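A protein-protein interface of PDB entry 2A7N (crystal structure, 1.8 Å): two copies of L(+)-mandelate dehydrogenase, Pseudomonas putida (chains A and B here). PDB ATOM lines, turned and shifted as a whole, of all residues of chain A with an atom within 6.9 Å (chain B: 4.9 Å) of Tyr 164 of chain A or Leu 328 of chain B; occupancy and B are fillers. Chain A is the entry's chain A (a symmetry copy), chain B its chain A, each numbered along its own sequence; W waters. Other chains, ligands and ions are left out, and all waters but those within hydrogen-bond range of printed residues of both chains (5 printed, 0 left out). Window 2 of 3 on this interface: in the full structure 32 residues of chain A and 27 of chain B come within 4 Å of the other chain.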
ATOM      1  N   GLY A  30      28.299  -0.580  -0.085  1.00  0.00           N
ATOM      2  CA  GLY A  30      27.919  -1.752   0.684  1.00  0.00           C
ATOM      3  C   GLY A  30      26.603  -2.290   0.149  1.00  0.00           C
ATOM      4  O   GLY A  30      26.037  -1.742  -0.798  1.00  0.00           O
ATOM      5  N   ALA A  31      26.109  -3.363   0.753  1.00  0.00           N
ATOM      6  CA  ALA A  31      24.856  -3.967   0.321  1.00  0.00           C
ATOM      7  C   ALA A  31      23.637  -3.168   0.779  1.00  0.00           C
ATOM      8  O   ALA A  31      23.613  -2.608   1.875  1.00  0.00           O
ATOM      9  CB  ALA A  31      24.765  -5.401   0.839  1.00  0.00           C
ATOM     10  N   GLU A  32      22.630  -3.129  -0.086  1.00  0.00           N
ATOM     11  CA  GLU A  32      21.366  -2.437   0.160  1.00  0.00           C
ATOM     12  C   GLU A  32      21.421  -1.096   0.905  1.00  0.00           C
ATOM     13  O   GLU A  32      21.971  -0.126   0.388  1.00  0.00           O
ATOM     14  CB  GLU A  32      20.395  -3.408   0.841  1.00  0.00           C
ATOM     15  CG  GLU A  32      20.340  -4.746   0.100  1.00  0.00           C
ATOM     16  CD  GLU A  32      19.179  -5.627   0.505  1.00  0.00           C
ATOM     17  OE1 GLU A  32      18.929  -5.779   1.717  1.00  0.00           O
ATOM     18  OE2 GLU A  32      18.522  -6.185  -0.400  1.00  0.00           O
ATOM     19  N   ASP A  33      20.859  -1.033   2.110  1.00  0.00           N
ATOM     20  CA  ASP A  33      20.821   0.222   2.870  1.00  0.00           C
ATOM     21  C   ASP A  33      22.136   0.661   3.499  1.00  0.00           C
ATOM     22  O   ASP A  33      22.236   1.763   4.048  1.00  0.00           O
ATOM     23  CB  ASP A  33      19.747   0.129   3.953  1.00  0.00           C
ATOM     24  CG  ASP A  33      18.381  -0.177   3.381  1.00  0.00           C
ATOM     25  OD1 ASP A  33      17.896   0.635   2.566  1.00  0.00           O
ATOM     26  OD2 ASP A  33      17.801  -1.227   3.737  1.00  0.00           O
ATOM     27  N   VAL A 161      26.220 -15.987  -4.049  1.00  0.00           N
ATOM     28  CA  VAL A 161      25.489 -15.170  -5.012  1.00  0.00           C
ATOM     29  C   VAL A 161      26.020 -13.762  -4.778  1.00  0.00           C
ATOM     30  O   VAL A 161      26.547 -13.468  -3.707  1.00  0.00           O
ATOM     31  CB  VAL A 161      23.954 -15.189  -4.780  1.00  0.00           C
ATOM     32  CG1 VAL A 161      23.430 -16.615  -4.886  1.00  0.00           C
ATOM     33  CG2 VAL A 161      23.611 -14.578  -3.422  1.00  0.00           C
ATOM     34  N   ASN A 162      25.895 -12.898  -5.778  1.00  0.00           N
ATOM     35  CA  ASN A 162      26.389 -11.529  -5.669  1.00  0.00           C
ATOM     36  C   ASN A 162      25.581 -10.665  -4.703  1.00  0.00           C
ATOM     37  O   ASN A 162      24.353 -10.758  -4.643  1.00  0.00           O
ATOM     38  CB  ASN A 162      26.402 -10.889  -7.058  1.00  0.00           C
ATOM     39  CG  ASN A 162      27.286 -11.647  -8.037  1.00  0.00           C
ATOM     40  OD1 ASN A 162      27.138 -11.525  -9.254  1.00  0.00           O
ATOM     41  ND2 ASN A 162      28.219 -12.430  -7.505  1.00  0.00           N
ATOM     42  N   GLY A 163      26.281  -9.832  -3.937  1.00  0.00           N
ATOM     43  CA  GLY A 163      25.604  -8.949  -3.007  1.00  0.00           C
ATOM     44  C   GLY A 163      24.817  -7.920  -3.796  1.00  0.00           C
ATOM     45  O   GLY A 163      25.184  -7.593  -4.926  1.00  0.00           O
ATOM     46  N   TYR A 164      23.735  -7.413  -3.217  1.00  0.00           N
ATOM     47  CA  TYR A 164      22.907  -6.417  -3.894  1.00  0.00           C
ATOM     48  C   TYR A 164      23.416  -5.015  -3.554  1.00  0.00           C
ATOM     49  O   TYR A 164      22.920  -4.365  -2.628  1.00  0.00           O
ATOM     50  CB  TYR A 164      21.448  -6.572  -3.454  1.00  0.00           C
ATOM     51  CG  TYR A 164      20.431  -5.965  -4.398  1.00  0.00           C
ATOM     52  CD1 TYR A 164      20.228  -6.499  -5.673  1.00  0.00           C
ATOM     53  CD2 TYR A 164      19.650  -4.876  -4.008  1.00  0.00           C
ATOM     54  CE1 TYR A 164      19.267  -5.971  -6.533  1.00  0.00           C
ATOM     55  CE2 TYR A 164      18.682  -4.336  -4.864  1.00  0.00           C
ATOM     56  CZ  TYR A 164      18.497  -4.889  -6.123  1.00  0.00           C
ATOM     57  OH  TYR A 164      17.534  -4.373  -6.966  1.00  0.00           O
ATOM     58  N   ARG A 165      24.413  -4.557  -4.306  1.00  0.00           N
ATOM     59  CA  ARG A 165      24.993  -3.243  -4.077  1.00  0.00           C
ATOM     60  C   ARG A 165      24.343  -2.243  -5.017  1.00  0.00           C
ATOM     61  O   ARG A 165      24.661  -2.169  -6.205  1.00  0.00           O
ATOM     62  CB  ARG A 165      26.510  -3.306  -4.267  1.00  0.00           C
ATOM     63  CG  ARG A 165      27.173  -4.259  -3.271  1.00  0.00           C
ATOM     64  CD  ARG A 165      28.648  -3.951  -3.074  1.00  0.00           C
ATOM     65  NE  ARG A 165      29.487  -4.467  -4.150  1.00  0.00           N
ATOM     66  CZ  ARG A 165      29.820  -5.746  -4.291  1.00  0.00           C
ATOM     67  NH1 ARG A 165      29.381  -6.652  -3.426  1.00  0.00           N
ATOM     68  NH2 ARG A 165      30.602  -6.117  -5.295  1.00  0.00           N
ATOM     69  N   GLU A 166      23.428  -1.464  -4.453  1.00  0.00           N
ATOM     70  CA  GLU A 166      22.652  -0.501  -5.215  1.00  0.00           C
ATOM     71  C   GLU A 166      23.415   0.675  -5.814  1.00  0.00           C
ATOM     72  O   GLU A 166      22.948   1.283  -6.778  1.00  0.00           O
ATOM     73  CB  GLU A 166      21.473  -0.045  -4.353  1.00  0.00           C
ATOM     74  CG  GLU A 166      20.693  -1.253  -3.834  1.00  0.00           C
ATOM     75  CD  GLU A 166      19.607  -0.915  -2.831  1.00  0.00           C
ATOM     76  OE1 GLU A 166      19.798   0.019  -2.025  1.00  0.00           O
ATOM     77  OE2 GLU A 166      18.569  -1.609  -2.830  1.00  0.00           O
ATOM     78  N   ARG A 167      24.582   1.004  -5.270  1.00  0.00           N
ATOM     79  CA  ARG A 167      25.357   2.093  -5.859  1.00  0.00           C
ATOM     80  C   ARG A 167      25.772   1.644  -7.260  1.00  0.00           C
ATOM     81  O   ARG A 167      25.699   2.418  -8.215  1.00  0.00           O
ATOM     82  CB  ARG A 167      26.618   2.400  -5.054  1.00  0.00           C
ATOM     83  CG  ARG A 167      26.394   2.922  -3.652  1.00  0.00           C
ATOM     84  CD  ARG A 167      27.670   3.581  -3.139  1.00  0.00           C
ATOM     85  NE  ARG A 167      27.606   3.880  -1.712  1.00  0.00           N
ATOM     86  CZ  ARG A 167      28.344   4.807  -1.110  1.00  0.00           C
ATOM     87  NH1 ARG A 167      29.205   5.538  -1.813  1.00  0.00           N
ATOM     88  NH2 ARG A 167      28.228   4.994   0.199  1.00  0.00           N
ATOM     89  N   LEU A 169      24.284  -0.530  -9.145  1.00  0.00           N
ATOM     90  CA  LEU A 169      23.088  -0.579  -9.980  1.00  0.00           C
ATOM     91  C   LEU A 169      22.744   0.814 -10.500  1.00  0.00           C
ATOM     92  O   LEU A 169      22.379   0.977 -11.662  1.00  0.00           O
ATOM     93  CB  LEU A 169      21.911  -1.152  -9.185  1.00  0.00           C
ATOM     94  CG  LEU A 169      22.057  -2.633  -8.828  1.00  0.00           C
ATOM     95  CD1 LEU A 169      20.952  -3.055  -7.870  1.00  0.00           C
ATOM     96  CD2 LEU A 169      22.020  -3.465 -10.106  1.00  0.00           C
ATOM     97  N   ARG A 258      29.569  -5.873   2.188  1.00  0.00           N
ATOM     98  CA  ARG A 258      29.218  -5.836   0.772  1.00  0.00           C
ATOM     99  C   ARG A 258      28.313  -6.966   0.275  1.00  0.00           C
ATOM    100  O   ARG A 258      27.879  -6.943  -0.879  1.00  0.00           O
ATOM    101  CB  ARG A 258      30.506  -5.814  -0.059  1.00  0.00           C
ATOM    102  CG  ARG A 258      31.376  -4.587   0.197  1.00  0.00           C
ATOM    103  CD  ARG A 258      32.808  -4.811  -0.269  1.00  0.00           C
ATOM    104  NE  ARG A 258      32.953  -4.915  -1.722  1.00  0.00           N
ATOM    105  CZ  ARG A 258      32.930  -3.881  -2.561  1.00  0.00           C
ATOM    106  NH1 ARG A 258      32.761  -2.644  -2.107  1.00  0.00           N
ATOM    107  NH2 ARG A 258      33.109  -4.082  -3.859  1.00  0.00           N
ATOM    108  N   GLN A 259      28.015  -7.937   1.133  1.00  0.00           N
ATOM    109  CA  GLN A 259      27.194  -9.075   0.724  1.00  0.00           C
ATOM    110  C   GLN A 259      25.798  -9.183   1.331  1.00  0.00           C
ATOM    111  O   GLN A 259      24.828  -9.452   0.622  1.00  0.00           O
ATOM    112  CB  GLN A 259      27.959 -10.376   0.994  1.00  0.00           C
ATOM    113  CG  GLN A 259      29.106 -10.612   0.029  1.00  0.00           C
ATOM    114  CD  GLN A 259      28.609 -10.854  -1.384  1.00  0.00           C
ATOM    115  OE1 GLN A 259      28.033 -11.901  -1.683  1.00  0.00           O
ATOM    116  NE2 GLN A 259      28.815  -9.879  -2.255  1.00  0.00           N
ATOM    117  N   LEU A 260      25.698  -8.985   2.639  1.00  0.00           N
ATOM    118  CA  LEU A 260      24.421  -9.089   3.338  1.00  0.00           C
ATOM    119  C   LEU A 260      24.372  -7.922   4.312  1.00  0.00           C
ATOM    120  O   LEU A 260      25.080  -7.917   5.317  1.00  0.00           O
ATOM    121  CB  LEU A 260      24.356 -10.427   4.085  1.00  0.00           C
ATOM    122  CG  LEU A 260      23.087 -10.789   4.858  1.00  0.00           C
ATOM    123  CD1 LEU A 260      21.891 -10.820   3.895  1.00  0.00           C
ATOM    124  CD2 LEU A 260      23.272 -12.150   5.529  1.00  0.00           C
ATOM    125  N   LEU B   5      14.784   2.062 -10.215  1.00  0.00           N
ATOM    126  CA  LEU B   5      13.800   1.391  -9.377  1.00  0.00           C
ATOM    127  C   LEU B   5      14.390   0.045  -8.972  1.00  0.00           C
ATOM    128  O   LEU B   5      14.126  -0.984  -9.597  1.00  0.00           O
ATOM    129  CB  LEU B   5      12.491   1.215 -10.153  1.00  0.00           C
ATOM    130  CG  LEU B   5      11.834   2.539 -10.575  1.00  0.00           C
ATOM    131  CD1 LEU B   5      10.686   2.274 -11.543  1.00  0.00           C
ATOM    132  CD2 LEU B   5      11.335   3.281  -9.343  1.00  0.00           C
ATOM    133  N   PHE B   6      15.194   0.064  -7.913  1.00  0.00           N
ATOM    134  CA  PHE B   6      15.860  -1.143  -7.446  1.00  0.00           C
ATOM    135  C   PHE B   6      15.361  -1.711  -6.120  1.00  0.00           C
ATOM    136  O   PHE B   6      15.800  -2.781  -5.707  1.00  0.00           O
ATOM    137  CB  PHE B   6      17.366  -0.879  -7.378  1.00  0.00           C
ATOM    138  CG  PHE B   6      17.956  -0.485  -8.705  1.00  0.00           C
ATOM    139  CD1 PHE B   6      18.019  -1.400  -9.751  1.00  0.00           C
ATOM    140  CD2 PHE B   6      18.436   0.803  -8.914  1.00  0.00           C
ATOM    141  CE1 PHE B   6      18.528  -1.030 -10.996  1.00  0.00           C
ATOM    142  CE2 PHE B   6      18.947   1.185 -10.155  1.00  0.00           C
ATOM    143  CZ  PHE B   6      19.003   0.265 -11.193  1.00  0.00           C
ATOM    144  N   ASN B   7      14.443  -1.006  -5.466  1.00  0.00           N
ATOM    145  CA  ASN B   7      13.882  -1.471  -4.200  1.00  0.00           C
ATOM    146  C   ASN B   7      12.565  -0.762  -3.887  1.00  0.00           C
ATOM    147  O   ASN B   7      12.136   0.123  -4.624  1.00  0.00           O
ATOM    148  CB  ASN B   7      14.874  -1.254  -3.050  1.00  0.00           C
ATOM    149  CG  ASN B   7      15.261   0.201  -2.875  1.00  0.00           C
ATOM    150  OD1 ASN B   7      14.409   1.092  -2.923  1.00  0.00           O
ATOM    151  ND2 ASN B   7      16.548   0.452  -2.656  1.00  0.00           N
ATOM    152  N   TYR B  11      10.262   2.994  -5.181  1.00  0.00           N
ATOM    153  CA  TYR B  11       8.884   3.115  -5.633  1.00  0.00           C
ATOM    154  C   TYR B  11       8.128   4.106  -4.768  1.00  0.00           C
ATOM    155  O   TYR B  11       7.233   4.795  -5.259  1.00  0.00           O
ATOM    156  CB  TYR B  11       8.172   1.756  -5.637  1.00  0.00           C
ATOM    157  CG  TYR B  11       8.518   0.938  -6.859  1.00  0.00           C
ATOM    158  CD1 TYR B  11       9.679   0.169  -6.900  1.00  0.00           C
ATOM    159  CD2 TYR B  11       7.734   1.013  -8.013  1.00  0.00           C
ATOM    160  CE1 TYR B  11      10.059  -0.500  -8.061  1.00  0.00           C
ATOM    161  CE2 TYR B  11       8.107   0.349  -9.186  1.00  0.00           C
ATOM    162  CZ  TYR B  11       9.268  -0.403  -9.200  1.00  0.00           C
ATOM    163  OH  TYR B  11       9.652  -1.048 -10.353  1.00  0.00           O
ATOM    164  N   ARG B 289      11.947  -4.508   3.252  1.00  0.00           N
ATOM    165  CA  ARG B 289      13.073  -5.238   2.659  1.00  0.00           C
ATOM    166  C   ARG B 289      12.873  -6.741   2.785  1.00  0.00           C
ATOM    167  O   ARG B 289      12.168  -7.205   3.677  1.00  0.00           O
ATOM    168  CB  ARG B 289      14.388  -4.882   3.366  1.00  0.00           C
ATOM    169  CG  ARG B 289      14.998  -3.523   3.025  1.00  0.00           C
ATOM    170  CD  ARG B 289      15.626  -3.496   1.633  1.00  0.00           C
ATOM    171  NE  ARG B 289      16.483  -2.320   1.453  1.00  0.00           N
ATOM    172  CZ  ARG B 289      17.140  -2.029   0.334  1.00  0.00           C
ATOM    173  NH1 ARG B 289      17.043  -2.824  -0.727  1.00  0.00           N
ATOM    174  NH2 ARG B 289      17.913  -0.945   0.278  1.00  0.00           N
ATOM    175  N   GLU B 324       6.488  -5.434 -10.560  1.00  0.00           N
ATOM    176  CA  GLU B 324       7.896  -5.118 -10.353  1.00  0.00           C
ATOM    177  C   GLU B 324       8.296  -5.188  -8.887  1.00  0.00           C
ATOM    178  O   GLU B 324       9.366  -5.709  -8.552  1.00  0.00           O
ATOM    179  CB  GLU B 324       8.210  -3.733 -10.931  1.00  0.00           C
ATOM    180  CG  GLU B 324       7.913  -3.634 -12.434  1.00  0.00           C
ATOM    181  CD  GLU B 324       8.119  -2.239 -13.008  1.00  0.00           C
ATOM    182  OE1 GLU B 324       8.046  -1.249 -12.249  1.00  0.00           O
ATOM    183  OE2 GLU B 324       8.338  -2.133 -14.231  1.00  0.00           O
ATOM    184  N   VAL B 325       7.445  -4.665  -8.011  1.00  0.00           N
ATOM    185  CA  VAL B 325       7.747  -4.697  -6.589  1.00  0.00           C
ATOM    186  C   VAL B 325       7.768  -6.145  -6.100  1.00  0.00           C
ATOM    187  O   VAL B 325       8.645  -6.534  -5.328  1.00  0.00           O
ATOM    188  CB  VAL B 325       6.721  -3.868  -5.779  1.00  0.00           C
ATOM    189  CG1 VAL B 325       6.889  -4.142  -4.289  1.00  0.00           C
ATOM    190  CG2 VAL B 325       6.923  -2.374  -6.059  1.00  0.00           C
ATOM    191  N   LEU B 326       6.816  -6.950  -6.560  1.00  0.00           N
ATOM    192  CA  LEU B 326       6.782  -8.349  -6.148  1.00  0.00           C
ATOM    193  C   LEU B 326       7.986  -9.097  -6.715  1.00  0.00           C
ATOM    194  O   LEU B 326       8.532  -9.986  -6.063  1.00  0.00           O
ATOM    195  CB  LEU B 326       5.478  -9.018  -6.599  1.00  0.00           C
ATOM    196  CG  LEU B 326       4.206  -8.543  -5.887  1.00  0.00           C
ATOM    197  CD1 LEU B 326       2.987  -9.182  -6.539  1.00  0.00           C
ATOM    198  CD2 LEU B 326       4.269  -8.914  -4.399  1.00  0.00           C
ATOM    199  N   THR B 327       8.406  -8.733  -7.924  1.00  0.00           N
ATOM    200  CA  THR B 327       9.561  -9.384  -8.530  1.00  0.00           C
ATOM    201  C   THR B 327      10.816  -9.039  -7.729  1.00  0.00           C
ATOM    202  O   THR B 327      11.624  -9.913  -7.423  1.00  0.00           O
ATOM    203  CB  THR B 327       9.759  -8.944 -10.001  1.00  0.00           C
ATOM    204  OG1 THR B 327       8.659  -9.417 -10.791  1.00  0.00           O
ATOM    205  CG2 THR B 327      11.056  -9.519 -10.564  1.00  0.00           C
ATOM    206  N   LEU B 328      10.972  -7.763  -7.385  1.00  0.00           N
ATOM    207  CA  LEU B 328      12.131  -7.327  -6.612  1.00  0.00           C
ATOM    208  C   LEU B 328      12.142  -7.991  -5.243  1.00  0.00           C
ATOM    209  O   LEU B 328      13.187  -8.443  -4.773  1.00  0.00           O
ATOM    210  CB  LEU B 328      12.124  -5.803  -6.432  1.00  0.00           C
ATOM    211  CG  LEU B 328      12.449  -4.933  -7.648  1.00  0.00           C
ATOM    212  CD1 LEU B 328      12.252  -3.468  -7.294  1.00  0.00           C
ATOM    213  CD2 LEU B 328      13.881  -5.186  -8.098  1.00  0.00           C
ATOM    214  N   LEU B 329      10.982  -8.050  -4.596  1.00  0.00           N
ATOM    215  CA  LEU B 329      10.909  -8.658  -3.273  1.00  0.00           C
ATOM    216  C   LEU B 329      11.195 -10.152  -3.324  1.00  0.00           C
ATOM    217  O   LEU B 329      11.845 -10.692  -2.430  1.00  0.00           O
ATOM    218  CB  LEU B 329       9.546  -8.386  -2.625  1.00  0.00           C
ATOM    219  CG  LEU B 329       9.365  -6.950  -2.106  1.00  0.00           C
ATOM    220  CD1 LEU B 329       7.959  -6.753  -1.562  1.00  0.00           C
ATOM    221  CD2 LEU B 329      10.395  -6.670  -1.012  1.00  0.00           C
ATOM    222  N   LYS B 330      10.732 -10.822  -4.374  1.00  0.00           N
ATOM    223  CA  LYS B 330      10.982 -12.256  -4.488  1.00  0.00           C
ATOM    224  C   LYS B 330      12.479 -12.512  -4.659  1.00  0.00           C
ATOM    225  O   LYS B 330      13.052 -13.376  -3.991  1.00  0.00           O
ATOM    226  CB  LYS B 330      10.221 -12.853  -5.673  1.00  0.00           C
ATOM    227  CG  LYS B 330      10.320 -14.371  -5.729  1.00  0.00           C
ATOM    228  CD  LYS B 330       9.499 -14.955  -6.859  1.00  0.00           C
ATOM    229  CE  LYS B 330       9.419 -16.465  -6.721  1.00  0.00           C
ATOM    230  NZ  LYS B 330       8.633 -17.072  -7.824  1.00  0.00           N
ATOM    231  N   ALA B 331      13.108 -11.753  -5.548  1.00  0.00           N
ATOM    232  CA  ALA B 331      14.537 -11.899  -5.803  1.00  0.00           C
ATOM    233  C   ALA B 331      15.341 -11.517  -4.560  1.00  0.00           C
ATOM    234  O   ALA B 331      16.423 -12.053  -4.320  1.00  0.00           O
ATOM    235  CB  ALA B 331      14.946 -11.027  -6.986  1.00  0.00           C
ATOM    236  N   ASP B 332      14.799 -10.582  -3.785  1.00  0.00           N
ATOM    237  CA  ASP B 332      15.421 -10.103  -2.552  1.00  0.00           C
ATOM    238  C   ASP B 332      15.397 -11.245  -1.524  1.00  0.00           C
ATOM    239  O   ASP B 332      16.413 -11.561  -0.901  1.00  0.00           O
ATOM    240  CB  ASP B 332      14.636  -8.885  -2.046  1.00  0.00           C
ATOM    241  CG  ASP B 332      15.258  -8.231  -0.822  1.00  0.00           C
ATOM    242  OD1 ASP B 332      16.203  -8.792  -0.235  1.00  0.00           O
ATOM    243  OD2 ASP B 332      14.781  -7.143  -0.442  1.00  0.00           O
ATOM    244  N   ARG B 335      17.715 -14.057  -2.733  1.00  0.00           N
ATOM    245  CA  ARG B 335      19.107 -13.671  -2.536  1.00  0.00           C
ATOM    246  C   ARG B 335      19.485 -13.808  -1.060  1.00  0.00           C
ATOM    247  O   ARG B 335      20.576 -14.284  -0.718  1.00  0.00           O
ATOM    248  CB  ARG B 335      19.294 -12.225  -3.004  1.00  0.00           C
ATOM    249  CG  ARG B 335      20.713 -11.709  -2.968  1.00  0.00           C
ATOM    250  CD  ARG B 335      20.784 -10.286  -3.511  1.00  0.00           C
ATOM    251  NE  ARG B 335      20.238 -10.181  -4.863  1.00  0.00           N
ATOM    252  CZ  ARG B 335      19.090  -9.576  -5.169  1.00  0.00           C
ATOM    253  NH1 ARG B 335      18.352  -9.015  -4.223  1.00  0.00           N
ATOM    254  NH2 ARG B 335      18.675  -9.533  -6.427  1.00  0.00           N
HETATM  255  O   HOH W   1      18.597  -8.687  -1.256  1.00  0.00           O
HETATM  256  O   HOH W   2      22.451 -11.730  -6.171  1.00  0.00           O
HETATM  257  O   HOH W   3      16.897  -7.389   2.096  1.00  0.00           O
HETATM  258  O   HOH W   4      16.134  -5.200  -1.633  1.00  0.00           O
HETATM  259  O   HOH W   5      15.623   1.153   1.427  1.00  0.00           O
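Of the 15 printed residues of chain A, 6 touch a printed residue of chain B.
Printed residues of chain A that touch a printed residue of chain B: Glu 32, Asp 33, Asn 162, Tyr 164, Glu 166 and Leu 169.
Hydrophobic or aromatic side chains of chain A within 4 Å of the printed part of chain B: Tyr 164 and Leu 169.
Among the printed residues, Asp or Glu carboxylates within 4 Å of a Lys or Arg side-chain nitrogen of the other chain: Glu 32 of chain A with Arg 289 of chain B (3.7 Å), Asp 33 of chain A with Arg 289 of chain B (2.8 Å) and Glu 166 of chain A with Arg 289 of chain B (2.9 Å).
The backbone carbonyl oxygen of Phe 6 of chain B lies within hydrogen-bond range of the side-chain hydroxyl of Tyr 164 of chain A, 2.7 Å away.
The side-chain amide nitrogen (ND2) of Asn 7 of chain B sits at hydrogen-bond distance from the side-chain carboxylate (OE2) of Glu 166 of chain A, at 2.9 Å.
NH1 of Arg 289 of chain B lies within salt-bridge range of OE2 of Glu 32 of chain A (3.7 Å).
NH2 of Arg 289 of chain B is in salt-bridge range of OD1 of Asp 33 of chain A, 2.8 Å away.
NH1 of Arg 289 of chain B lies within salt-bridge range of OE2 of Glu 166 of chain A (2.9 Å).
OE2 of Glu 32 of chain A sits close to OD1 of Asp 332 of chain B.
Among the printed residues, merely in contact across the chains: Tyr 164 of chain A with Arg 335 of chain B, Leu 169 of chain A with Phe 6 of chain B, Asn 162 of chain A with Arg 335 of chain B and Tyr 164 of chain A with Leu 328 of chain B.
Water W5 bridges OD1 of Asp 33 of chain A (2.6 Å) and NH2 of Arg 289 of chain B (3.3 Å).
Water W1 lies within hydrogen-bond range of OD1 of Asp 332 of chain B, OE2 of Glu 32 of chain A and NH1 of Arg 335 of chain B.
Water W3 bridges the side-chain carboxylate of Glu 32 of chain A (2.6 Å) and the side-chain carboxylate of Asp 332 of chain B (2.8 Å).
Water W2 lies within hydrogen-bond range of the backbone carbonyl oxygen of Asn 162 of chain A and the guanidinium group of Arg 335 of chain B.
Water W4 lies within hydrogen-bond range of the side-chain carboxylate (OD2) of Asp 332 of chain B, the guanidinium group (NH1) of Arg 289 of chain B and the side-chain carboxylate (OE2) of Glu 32 of chain A.
Of chain B, only Phe 6, Leu 328 and Arg 335 come within 4 Å of Tyr 164 of chain A.
Of the printed residues of chain B, Leu 169 of chain A touches Phe 6 (3.5 Å).
Printed residues of chain A within 4 Å of Phe 6 of chain B: Tyr 164 (2.7 Å) and Leu 169 (3.5 Å).
Of chain A, only Tyr 164 (3.9 Å) comes within 4 Å of Leu 328 of chain B.
Printed residues of chain A within 4 Å of Arg 335 of chain B: Asn 162 (3.8 Å) and Tyr 164 (3.3 Å).
The backbone NH (N) of Glu 32 of chain A lies within hydrogen-bond range of the backbone carbonyl oxygen (O) of Tyr 164 of chain A.
No position is printed for both chains.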
